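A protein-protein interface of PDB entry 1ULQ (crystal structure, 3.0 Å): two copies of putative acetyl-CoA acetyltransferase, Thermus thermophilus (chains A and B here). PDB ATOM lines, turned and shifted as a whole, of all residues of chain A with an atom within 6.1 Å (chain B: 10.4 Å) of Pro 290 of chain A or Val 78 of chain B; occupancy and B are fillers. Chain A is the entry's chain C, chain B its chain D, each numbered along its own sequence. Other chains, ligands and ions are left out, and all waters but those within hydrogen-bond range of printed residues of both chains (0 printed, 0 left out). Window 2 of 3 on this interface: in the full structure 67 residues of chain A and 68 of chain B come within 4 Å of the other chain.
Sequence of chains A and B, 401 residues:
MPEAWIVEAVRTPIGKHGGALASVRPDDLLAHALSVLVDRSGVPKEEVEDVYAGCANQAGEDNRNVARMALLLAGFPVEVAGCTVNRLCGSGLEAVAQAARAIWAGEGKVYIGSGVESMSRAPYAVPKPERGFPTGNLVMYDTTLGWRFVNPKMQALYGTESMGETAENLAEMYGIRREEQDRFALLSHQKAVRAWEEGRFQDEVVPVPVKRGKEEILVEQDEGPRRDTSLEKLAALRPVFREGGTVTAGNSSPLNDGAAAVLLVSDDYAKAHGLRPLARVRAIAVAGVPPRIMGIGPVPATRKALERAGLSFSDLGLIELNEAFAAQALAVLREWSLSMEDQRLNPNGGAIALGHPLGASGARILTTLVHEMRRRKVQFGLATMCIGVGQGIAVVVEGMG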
ATOM      1  N   TYR A 158     -34.715  10.916  11.158  1.00  0.00           N
ATOM      2  CA  TYR A 158     -35.280   9.995  12.155  1.00  0.00           C
ATOM      3  C   TYR A 158     -36.486  10.798  12.609  1.00  0.00           C
ATOM      4  O   TYR A 158     -36.543  12.008  12.390  1.00  0.00           O
ATOM      5  CB  TYR A 158     -34.322   9.783  13.341  1.00  0.00           C
ATOM      6  CG  TYR A 158     -32.866   9.614  12.939  1.00  0.00           C
ATOM      7  CD1 TYR A 158     -32.121  10.699  12.474  1.00  0.00           C
ATOM      8  CD2 TYR A 158     -32.260   8.357  12.943  1.00  0.00           C
ATOM      9  CE1 TYR A 158     -30.825  10.538  12.016  1.00  0.00           C
ATOM     10  CE2 TYR A 158     -30.955   8.186  12.484  1.00  0.00           C
ATOM     11  CZ  TYR A 158     -30.246   9.280  12.020  1.00  0.00           C
ATOM     12  OH  TYR A 158     -28.963   9.117  11.533  1.00  0.00           O
ATOM     13  N   ALA A 287     -22.576   3.634  24.280  1.00  0.00           N
ATOM     14  CA  ALA A 287     -22.914   3.150  22.952  1.00  0.00           C
ATOM     15  C   ALA A 287     -24.167   3.806  22.399  1.00  0.00           C
ATOM     16  O   ALA A 287     -25.028   4.256  23.159  1.00  0.00           O
ATOM     17  CB  ALA A 287     -23.096   1.651  22.992  1.00  0.00           C
ATOM     18  N   GLY A 288     -24.265   3.858  21.070  1.00  0.00           N
ATOM     19  CA  GLY A 288     -25.432   4.441  20.431  1.00  0.00           C
ATOM     20  C   GLY A 288     -26.294   3.392  19.745  1.00  0.00           C
ATOM     21  O   GLY A 288     -25.802   2.381  19.250  1.00  0.00           O
ATOM     22  N   VAL A 289     -27.598   3.627  19.732  1.00  0.00           N
ATOM     23  CA  VAL A 289     -28.548   2.724  19.090  1.00  0.00           C
ATOM     24  C   VAL A 289     -29.513   3.631  18.344  1.00  0.00           C
ATOM     25  O   VAL A 289     -29.519   4.839  18.570  1.00  0.00           O
ATOM     26  CB  VAL A 289     -29.317   1.898  20.131  1.00  0.00           C
ATOM     27  CG1 VAL A 289     -28.343   1.050  20.926  1.00  0.00           C
ATOM     28  CG2 VAL A 289     -30.107   2.826  21.058  1.00  0.00           C
ATOM     29  N   PRO A 290     -30.335   3.074  17.446  1.00  0.00           N
ATOM     30  CA  PRO A 290     -31.288   3.894  16.690  1.00  0.00           C
ATOM     31  C   PRO A 290     -32.325   4.575  17.584  1.00  0.00           C
ATOM     32  O   PRO A 290     -32.943   3.940  18.433  1.00  0.00           O
ATOM     33  CB  PRO A 290     -31.899   2.896  15.712  1.00  0.00           C
ATOM     34  CG  PRO A 290     -31.884   1.638  16.490  1.00  0.00           C
ATOM     35  CD  PRO A 290     -30.505   1.652  17.118  1.00  0.00           C
ATOM     36  N   PRO A 291     -32.529   5.885  17.394  1.00  0.00           N
ATOM     37  CA  PRO A 291     -33.481   6.682  18.171  1.00  0.00           C
ATOM     38  C   PRO A 291     -34.836   6.020  18.396  1.00  0.00           C
ATOM     39  O   PRO A 291     -35.322   5.954  19.527  1.00  0.00           O
ATOM     40  CB  PRO A 291     -33.600   7.963  17.351  1.00  0.00           C
ATOM     41  CG  PRO A 291     -32.234   8.096  16.762  1.00  0.00           C
ATOM     42  CD  PRO A 291     -31.961   6.688  16.298  1.00  0.00           C
ATOM     43  N   ARG A 292     -35.441   5.525  17.322  1.00  0.00           N
ATOM     44  CA  ARG A 292     -36.753   4.903  17.418  1.00  0.00           C
ATOM     45  C   ARG A 292     -36.907   3.750  18.429  1.00  0.00           C
ATOM     46  O   ARG A 292     -38.034   3.319  18.711  1.00  0.00           O
ATOM     47  CB  ARG A 292     -37.201   4.450  16.036  1.00  0.00           C
ATOM     48  CG  ARG A 292     -36.229   3.545  15.328  1.00  0.00           C
ATOM     49  CD  ARG A 292     -36.998   2.357  14.819  1.00  0.00           C
ATOM     50  NE  ARG A 292     -38.344   2.764  14.432  1.00  0.00           N
ATOM     51  CZ  ARG A 292     -39.419   1.997  14.557  1.00  0.00           C
ATOM     52  NH1 ARG A 292     -39.316   0.767  15.059  1.00  0.00           N
ATOM     53  NH2 ARG A 292     -40.606   2.471  14.199  1.00  0.00           N
ATOM     54  N   ILE A 293     -35.794   3.249  18.966  1.00  0.00           N
ATOM     55  CA  ILE A 293     -35.836   2.171  19.955  1.00  0.00           C
ATOM     56  C   ILE A 293     -34.723   2.363  20.970  1.00  0.00           C
ATOM     57  O   ILE A 293     -34.057   1.397  21.366  1.00  0.00           O
ATOM     58  CB  ILE A 293     -35.668   0.775  19.317  1.00  0.00           C
ATOM     59  CG1 ILE A 293     -34.311   0.686  18.602  1.00  0.00           C
ATOM     60  CG2 ILE A 293     -36.845   0.496  18.399  1.00  0.00           C
ATOM     61  CD1 ILE A 293     -34.039  -0.629  17.904  1.00  0.00           C
ATOM     62  N   MET A 294     -34.529   3.615  21.387  1.00  0.00           N
ATOM     63  CA  MET A 294     -33.491   3.983  22.353  1.00  0.00           C
ATOM     64  C   MET A 294     -33.488   3.079  23.573  1.00  0.00           C
ATOM     65  O   MET A 294     -32.481   2.936  24.245  1.00  0.00           O
ATOM     66  CB  MET A 294     -33.694   5.424  22.804  1.00  0.00           C
ATOM     67  CG  MET A 294     -35.063   5.666  23.402  1.00  0.00           C
ATOM     68  SD  MET A 294     -35.001   6.131  25.134  1.00  0.00           S
ATOM     69  CE  MET A 294     -35.297   4.579  25.957  1.00  0.00           C
ATOM     70  N   GLY A 295     -34.627   2.466  23.849  1.00  0.00           N
ATOM     71  CA  GLY A 295     -34.742   1.596  25.001  1.00  0.00           C
ATOM     72  C   GLY A 295     -33.677   0.534  25.174  1.00  0.00           C
ATOM     73  O   GLY A 295     -33.255   0.274  26.306  1.00  0.00           O
ATOM     74  N   ILE A 296     -33.224  -0.085  24.088  1.00  0.00           N
ATOM     75  CA  ILE A 296     -32.219  -1.144  24.230  1.00  0.00           C
ATOM     76  C   ILE A 296     -30.801  -0.668  24.507  1.00  0.00           C
ATOM     77  O   ILE A 296     -29.910  -1.481  24.740  1.00  0.00           O
ATOM     78  CB  ILE A 296     -32.159  -2.071  23.002  1.00  0.00           C
ATOM     79  CG1 ILE A 296     -32.234  -1.229  21.738  1.00  0.00           C
ATOM     80  CG2 ILE A 296     -33.211  -3.162  23.114  1.00  0.00           C
ATOM     81  CD1 ILE A 296     -31.910  -2.002  20.496  1.00  0.00           C
ATOM     82  N   VAL A 389     -33.005   9.697  22.479  1.00  0.00           N
ATOM     83  CA  VAL A 389     -32.498   9.917  21.129  1.00  0.00           C
ATOM     84  C   VAL A 389     -31.506   8.833  20.707  1.00  0.00           C
ATOM     85  O   VAL A 389     -30.718   9.033  19.778  1.00  0.00           O
ATOM     86  CB  VAL A 389     -31.833  11.311  20.949  1.00  0.00           C
ATOM     87  CG1 VAL A 389     -31.584  11.567  19.485  1.00  0.00           C
ATOM     88  CG2 VAL A 389     -32.719  12.407  21.495  1.00  0.00           C
ATOM     89  N   GLY A 390     -31.537   7.697  21.411  1.00  0.00           N
ATOM     90  CA  GLY A 390     -30.704   6.547  21.061  1.00  0.00           C
ATOM     91  C   GLY A 390     -29.299   6.292  21.583  1.00  0.00           C
ATOM     92  O   GLY A 390     -28.359   6.219  20.790  1.00  0.00           O
ATOM     93  N   LYS B  45     -16.906   7.659   9.468  1.00  0.00           N
ATOM     94  CA  LYS B  45     -17.688   8.064  10.625  1.00  0.00           C
ATOM     95  C   LYS B  45     -17.967   6.921  11.586  1.00  0.00           C
ATOM     96  O   LYS B  45     -17.849   7.099  12.797  1.00  0.00           O
ATOM     97  CB  LYS B  45     -19.013   8.702  10.180  1.00  0.00           C
ATOM     98  CG  LYS B  45     -18.873  10.122   9.643  1.00  0.00           C
ATOM     99  CD  LYS B  45     -20.148  10.590   8.973  1.00  0.00           C
ATOM    100  CE  LYS B  45     -19.921  11.894   8.241  1.00  0.00           C
ATOM    101  NZ  LYS B  45     -20.828  12.049   7.062  1.00  0.00           N
ATOM    102  N   GLU B  46     -18.330   5.755  11.063  1.00  0.00           N
ATOM    103  CA  GLU B  46     -18.627   4.613  11.923  1.00  0.00           C
ATOM    104  C   GLU B  46     -17.479   4.256  12.861  1.00  0.00           C
ATOM    105  O   GLU B  46     -17.651   3.461  13.782  1.00  0.00           O
ATOM    106  CB  GLU B  46     -18.985   3.395  11.083  1.00  0.00           C
ATOM    107  CG  GLU B  46     -18.193   3.314   9.806  1.00  0.00           C
ATOM    108  CD  GLU B  46     -17.834   1.897   9.439  1.00  0.00           C
ATOM    109  OE1 GLU B  46     -18.756   1.046   9.385  1.00  0.00           O
ATOM    110  OE2 GLU B  46     -16.624   1.649   9.201  1.00  0.00           O
ATOM    111  N   GLU B  47     -16.308   4.841  12.632  1.00  0.00           N
ATOM    112  CA  GLU B  47     -15.143   4.574  13.476  1.00  0.00           C
ATOM    113  C   GLU B  47     -15.166   5.383  14.760  1.00  0.00           C
ATOM    114  O   GLU B  47     -14.544   5.002  15.746  1.00  0.00           O
ATOM    115  CB  GLU B  47     -13.841   4.882  12.720  1.00  0.00           C
ATOM    116  CG  GLU B  47     -13.513   3.908  11.595  1.00  0.00           C
ATOM    117  CD  GLU B  47     -13.317   2.485  12.086  1.00  0.00           C
ATOM    118  OE1 GLU B  47     -13.472   1.557  11.265  1.00  0.00           O
ATOM    119  OE2 GLU B  47     -13.004   2.296  13.282  1.00  0.00           O
ATOM    120  N   VAL B  48     -15.868   6.507  14.742  1.00  0.00           N
ATOM    121  CA  VAL B  48     -15.959   7.360  15.918  1.00  0.00           C
ATOM    122  C   VAL B  48     -16.768   6.714  17.053  1.00  0.00           C
ATOM    123  O   VAL B  48     -17.918   6.309  16.875  1.00  0.00           O
ATOM    124  CB  VAL B  48     -16.567   8.705  15.555  1.00  0.00           C
ATOM    125  CG1 VAL B  48     -16.553   9.626  16.763  1.00  0.00           C
ATOM    126  CG2 VAL B  48     -15.774   9.314  14.431  1.00  0.00           C
ATOM    127  N   GLU B  49     -16.146   6.640  18.224  1.00  0.00           N
ATOM    128  CA  GLU B  49     -16.735   6.022  19.407  1.00  0.00           C
ATOM    129  C   GLU B  49     -17.745   6.877  20.152  1.00  0.00           C
ATOM    130  O   GLU B  49     -18.838   6.418  20.486  1.00  0.00           O
ATOM    131  CB  GLU B  49     -15.612   5.640  20.375  1.00  0.00           C
ATOM    132  CG  GLU B  49     -16.051   5.181  21.749  1.00  0.00           C
ATOM    133  CD  GLU B  49     -16.419   3.726  21.771  1.00  0.00           C
ATOM    134  OE1 GLU B  49     -15.751   2.947  21.066  1.00  0.00           O
ATOM    135  OE2 GLU B  49     -17.354   3.345  22.500  1.00  0.00           O
ATOM    136  N   ASP B  50     -17.373   8.122  20.413  1.00  0.00           N
ATOM    137  CA  ASP B  50     -18.220   9.016  21.175  1.00  0.00           C
ATOM    138  C   ASP B  50     -17.865  10.437  20.764  1.00  0.00           C
ATOM    139  O   ASP B  50     -16.755  10.690  20.293  1.00  0.00           O
ATOM    140  CB  ASP B  50     -17.922   8.769  22.653  1.00  0.00           C
ATOM    141  CG  ASP B  50     -18.806   9.553  23.582  1.00  0.00           C
ATOM    142  OD1 ASP B  50     -19.825  10.105  23.109  1.00  0.00           O
ATOM    143  OD2 ASP B  50     -18.475   9.595  24.795  1.00  0.00           O
ATOM    144  N   VAL B  51     -18.805  11.363  20.922  1.00  0.00           N
ATOM    145  CA  VAL B  51     -18.557  12.750  20.545  1.00  0.00           C
ATOM    146  C   VAL B  51     -18.899  13.703  21.686  1.00  0.00           C
ATOM    147  O   VAL B  51     -20.055  13.804  22.111  1.00  0.00           O
ATOM    148  CB  VAL B  51     -19.374  13.141  19.274  1.00  0.00           C
ATOM    149  CG1 VAL B  51     -19.150  14.602  18.918  1.00  0.00           C
ATOM    150  CG2 VAL B  51     -18.962  12.257  18.114  1.00  0.00           C
ATOM    151  N   ALA B  67     -24.565  17.414  21.075  1.00  0.00           N
ATOM    152  CA  ALA B  67     -23.610  16.484  20.483  1.00  0.00           C
ATOM    153  C   ALA B  67     -24.313  15.361  19.738  1.00  0.00           C
ATOM    154  O   ALA B  67     -24.010  15.104  18.570  1.00  0.00           O
ATOM    155  CB  ALA B  67     -22.692  15.910  21.542  1.00  0.00           C
ATOM    156  N   ARG B  68     -25.262  14.703  20.402  1.00  0.00           N
ATOM    157  CA  ARG B  68     -25.973  13.601  19.769  1.00  0.00           C
ATOM    158  C   ARG B  68     -26.845  14.083  18.608  1.00  0.00           C
ATOM    159  O   ARG B  68     -26.938  13.420  17.570  1.00  0.00           O
ATOM    160  CB  ARG B  68     -26.813  12.853  20.795  1.00  0.00           C
ATOM    161  CG  ARG B  68     -27.659  11.729  20.213  1.00  0.00           C
ATOM    162  CD  ARG B  68     -26.874  10.644  19.474  1.00  0.00           C
ATOM    163  NE  ARG B  68     -27.714   9.457  19.284  1.00  0.00           N
ATOM    164  CZ  ARG B  68     -27.356   8.363  18.617  1.00  0.00           C
ATOM    165  NH1 ARG B  68     -26.153   8.284  18.052  1.00  0.00           N
ATOM    166  NH2 ARG B  68     -28.197   7.339  18.519  1.00  0.00           N
ATOM    167  N   MET B  69     -27.470  15.242  18.769  1.00  0.00           N
ATOM    168  CA  MET B  69     -28.304  15.783  17.705  1.00  0.00           C
ATOM    169  C   MET B  69     -27.435  16.158  16.496  1.00  0.00           C
ATOM    170  O   MET B  69     -27.752  15.834  15.349  1.00  0.00           O
ATOM    171  CB  MET B  69     -29.041  17.023  18.203  1.00  0.00           C
ATOM    172  CG  MET B  69     -29.817  16.793  19.473  1.00  0.00           C
ATOM    173  SD  MET B  69     -31.391  15.914  19.300  1.00  0.00           S
ATOM    174  CE  MET B  69     -32.293  16.620  20.690  1.00  0.00           C
ATOM    175  N   LEU B  71     -24.373  15.105  15.672  1.00  0.00           N
ATOM    176  CA  LEU B  71     -23.734  13.959  15.039  1.00  0.00           C
ATOM    177  C   LEU B  71     -24.721  13.185  14.148  1.00  0.00           C
ATOM    178  O   LEU B  71     -24.351  12.715  13.066  1.00  0.00           O
ATOM    179  CB  LEU B  71     -23.101  13.071  16.112  1.00  0.00           C
ATOM    180  CG  LEU B  71     -23.421  11.583  16.198  1.00  0.00           C
ATOM    181  CD1 LEU B  71     -22.455  10.951  17.165  1.00  0.00           C
ATOM    182  CD2 LEU B  71     -24.849  11.347  16.663  1.00  0.00           C
ATOM    183  N   LEU B  72     -25.976  13.060  14.581  1.00  0.00           N
ATOM    184  CA  LEU B  72     -26.974  12.374  13.757  1.00  0.00           C
ATOM    185  C   LEU B  72     -27.257  13.224  12.511  1.00  0.00           C
ATOM    186  O   LEU B  72     -27.337  12.695  11.395  1.00  0.00           O
ATOM    187  CB  LEU B  72     -28.280  12.148  14.533  1.00  0.00           C
ATOM    188  CG  LEU B  72     -28.349  10.925  15.448  1.00  0.00           C
ATOM    189  CD1 LEU B  72     -29.768  10.714  15.913  1.00  0.00           C
ATOM    190  CD2 LEU B  72     -27.891   9.699  14.698  1.00  0.00           C
ATOM    191  N   LEU B  73     -27.384  14.536  12.718  1.00  0.00           N
ATOM    192  CA  LEU B  73     -27.651  15.476  11.641  1.00  0.00           C
ATOM    193  C   LEU B  73     -26.543  15.442  10.614  1.00  0.00           C
ATOM    194  O   LEU B  73     -26.795  15.559   9.413  1.00  0.00           O
ATOM    195  CB  LEU B  73     -27.808  16.898  12.198  1.00  0.00           C
ATOM    196  CG  LEU B  73     -29.176  17.211  12.834  1.00  0.00           C
ATOM    197  CD1 LEU B  73     -29.067  18.351  13.821  1.00  0.00           C
ATOM    198  CD2 LEU B  73     -30.178  17.544  11.743  1.00  0.00           C
ATOM    199  N   ALA B  74     -25.318  15.256  11.096  1.00  0.00           N
ATOM    200  CA  ALA B  74     -24.139  15.219  10.236  1.00  0.00           C
ATOM    201  C   ALA B  74     -24.006  13.923   9.450  1.00  0.00           C
ATOM    202  O   ALA B  74     -23.050  13.735   8.703  1.00  0.00           O
ATOM    203  CB  ALA B  74     -22.893  15.456  11.063  1.00  0.00           C
ATOM    204  N   GLY B  75     -24.961  13.021   9.625  1.00  0.00           N
ATOM    205  CA  GLY B  75     -24.912  11.782   8.881  1.00  0.00           C
ATOM    206  C   GLY B  75     -24.158  10.640   9.510  1.00  0.00           C
ATOM    207  O   GLY B  75     -23.997   9.604   8.873  1.00  0.00           O
ATOM    208  N   PHE B  76     -23.692  10.810  10.745  1.00  0.00           N
ATOM    209  CA  PHE B  76     -22.967   9.733  11.426  1.00  0.00           C
ATOM    210  C   PHE B  76     -23.898   8.571  11.711  1.00  0.00           C
ATOM    211  O   PHE B  76     -25.077   8.771  11.992  1.00  0.00           O
ATOM    212  CB  PHE B  76     -22.395  10.211  12.753  1.00  0.00           C
ATOM    213  CG  PHE B  76     -21.228  11.133  12.617  1.00  0.00           C
ATOM    214  CD1 PHE B  76     -21.326  12.293  11.860  1.00  0.00           C
ATOM    215  CD2 PHE B  76     -20.036  10.858  13.278  1.00  0.00           C
ATOM    216  CE1 PHE B  76     -20.252  13.169  11.764  1.00  0.00           C
ATOM    217  CE2 PHE B  76     -18.954  11.726  13.191  1.00  0.00           C
ATOM    218  CZ  PHE B  76     -19.061  12.887  12.433  1.00  0.00           C
ATOM    219  N   PRO B  77     -23.387   7.339  11.638  1.00  0.00           N
ATOM    220  CA  PRO B  77     -24.247   6.193  11.909  1.00  0.00           C
ATOM    221  C   PRO B  77     -24.809   6.263  13.333  1.00  0.00           C
ATOM    222  O   PRO B  77     -24.249   6.928  14.214  1.00  0.00           O
ATOM    223  CB  PRO B  77     -23.319   5.004  11.674  1.00  0.00           C
ATOM    224  CG  PRO B  77     -21.990   5.536  12.001  1.00  0.00           C
ATOM    225  CD  PRO B  77     -22.013   6.898  11.356  1.00  0.00           C
ATOM    226  N   VAL B  78     -25.920   5.572  13.547  1.00  0.00           N
ATOM    227  CA  VAL B  78     -26.603   5.580  14.829  1.00  0.00           C
ATOM    228  C   VAL B  78     -25.806   5.085  16.055  1.00  0.00           C
ATOM    229  O   VAL B  78     -26.114   5.447  17.193  1.00  0.00           O
ATOM    230  CB  VAL B  78     -27.922   4.802  14.678  1.00  0.00           C
ATOM    231  CG1 VAL B  78     -27.982   3.662  15.653  1.00  0.00           C
ATOM    232  CG2 VAL B  78     -29.072   5.732  14.856  1.00  0.00           C
ATOM    233  N   GLU B  79     -24.777   4.279  15.826  1.00  0.00           N
ATOM    234  CA  GLU B  79     -23.982   3.744  16.933  1.00  0.00           C
ATOM    235  C   GLU B  79     -23.034   4.730  17.629  1.00  0.00           C
ATOM    236  O   GLU B  79     -22.655   4.510  18.781  1.00  0.00           O
ATOM    237  CB  GLU B  79     -23.176   2.532  16.470  1.00  0.00           C
ATOM    238  CG  GLU B  79     -24.016   1.388  15.956  1.00  0.00           C
ATOM    239  CD  GLU B  79     -24.442   1.580  14.510  1.00  0.00           C
ATOM    240  OE1 GLU B  79     -24.111   2.641  13.933  1.00  0.00           O
ATOM    241  OE2 GLU B  79     -25.104   0.670  13.951  1.00  0.00           O
ATOM    242  N   VAL B  80     -22.643   5.800  16.940  1.00  0.00           N
ATOM    243  CA  VAL B  80     -21.746   6.782  17.532  1.00  0.00           C
ATOM    244  C   VAL B  80     -22.482   7.457  18.667  1.00  0.00           C
ATOM    245  O   VAL B  80     -23.604   7.921  18.489  1.00  0.00           O
ATOM    246  CB  VAL B  80     -21.335   7.866  16.522  1.00  0.00           C
ATOM    247  CG1 VAL B  80     -20.164   8.681  17.072  1.00  0.00           C
ATOM    248  CG2 VAL B  80     -20.975   7.230  15.200  1.00  0.00           C
ATOM    249  N   ALA B  81     -21.860   7.512  19.837  1.00  0.00           N
ATOM    250  CA  ALA B  81     -22.498   8.147  20.983  1.00  0.00           C
ATOM    251  C   ALA B  81     -22.131   9.613  21.039  1.00  0.00           C
ATOM    252  O   ALA B  81     -21.338  10.093  20.230  1.00  0.00           O
ATOM    253  CB  ALA B  81     -22.070   7.469  22.258  1.00  0.00           C
ATOM    254  N   GLY B  82     -22.699  10.319  22.007  1.00  0.00           N
ATOM    255  CA  GLY B  82     -22.416  11.732  22.144  1.00  0.00           C
ATOM    256  C   GLY B  82     -22.855  12.259  23.492  1.00  0.00           C
ATOM    257  O   GLY B  82     -23.750  11.706  24.123  1.00  0.00           O
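O of Glu 79 of chain B is in hydrogen-bond range of N of Gly 288 of chain A (2.9 Å).
The backbone carbonyl oxygen (O) of Val 289 of chain A sits at hydrogen-bond distance from the guanidinium group (NH2) of Arg 68 of chain B (2.8 Å).
N of Val 289 of chain A lies within hydrogen-bond range of O of Val 78 of chain B, at 3.5 Å.
The backbone carbonyl oxygen of Val 389 of chain A is in hydrogen-bond range of the guanidinium group of Arg 68 of chain B (3.1 Å).
The backbone carbonyl oxygen (O) of Gly 390 of chain A lies within hydrogen-bond range of the guanidinium group (NH2) of Arg 68 of chain B, at 2.5 Å.
Of the 22 printed residues of chain B, 5 touch a printed residue of chain A.
Hydrophobic or aromatic side chains of chain B that line the printed part of chain A: Leu 72 and Val 78.
Hydrophobic or aromatic side chains of chain A within 4 Å of the printed part of chain B: Tyr 158, Pro 290, Pro 291 and Val 389.
Along chain A the printed residues that touch a printed residue of chain B span positions 158 to 390.
Among the printed residues, 13 pairs touch across the chains.
Among the printed residues, no Asp or Glu carboxylate lies within 4 Å of a Lys or Arg side-chain nitrogen of the other chain.
Among the printed residues, pairs that only touch across the chains: Pro 290 of chain A with Val 78 of chain B (3.0 Å), Gly 288 of chain A with Val 78 of chain B (3.3 Å), Pro 291 of chain A with Val 78 of chain B (3.4 Å), Tyr 158 of chain A with Leu 72 of chain B (3.4 Å), Pro 291 of chain A with Leu 72 of chain B (3.7 Å), Tyr 158 of chain A with Val 78 of chain B (3.9 Å), Tyr 158 of chain A with Phe 76 of chain B (3.9 Å) and Ala 287 of chain A with Glu 79 of chain B (3.98 Å).
Pro 290 of chain A touches just one residue of chain B: Val 78.
Of chain A, only Tyr 158, Gly 288, Val 289, Pro 290 and Pro 291 come within 4 Å of Val 78 of chain B.
Of chain B, only Arg 68 and Val 78 come within 4 Å of Val 289 of chain A.
No residue of chain B comes within 4 Å of Ile 293 of chain A.
Of chain B, only Arg 68 comes within 4 Å of Gly 390 of chain A.
Printed residues of chain A within 4 Å of Glu 79 of chain B: Ala 287 (3.98 Å) and Gly 288 (2.9 Å).
Of the printed residues of chain B, Tyr 158 of chain A touches Leu 72 (3.4 Å), Phe 76 (3.9 Å) and Val 78 (3.9 Å).
Of the printed residues of chain B, Ala 287 of chain A touches Glu 79 (3.98 Å).
The nearest printed residue of chain A that does not touch Leu 72 of chain B is Val 389 of chain A (4.1 Å).
The backbone carbonyl oxygen (O) of Gly 390 of chain A is in hydrogen-bond range of the backbone NH (N) of Val 289 of chain A (2.9 Å).
NH1 of Arg 68 of chain B is in hydrogen-bond range of O of Val 78 of chain B.
The backbone carbonyl oxygen (O) of Val 80 of chain B sits at hydrogen-bond distance from the guanidinium group (NH1) of Arg 68 of chain B (2.6 Å).
The backbone NH (N) of Phe 76 of chain B sits at hydrogen-bond distance from the backbone carbonyl oxygen (O) of Leu 71 of chain B (3.1 Å).
No position is printed for both chains.
Of the 13 pairs that touch across the chains among the printed residues, none has its exchanged pair printed and touching as well.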
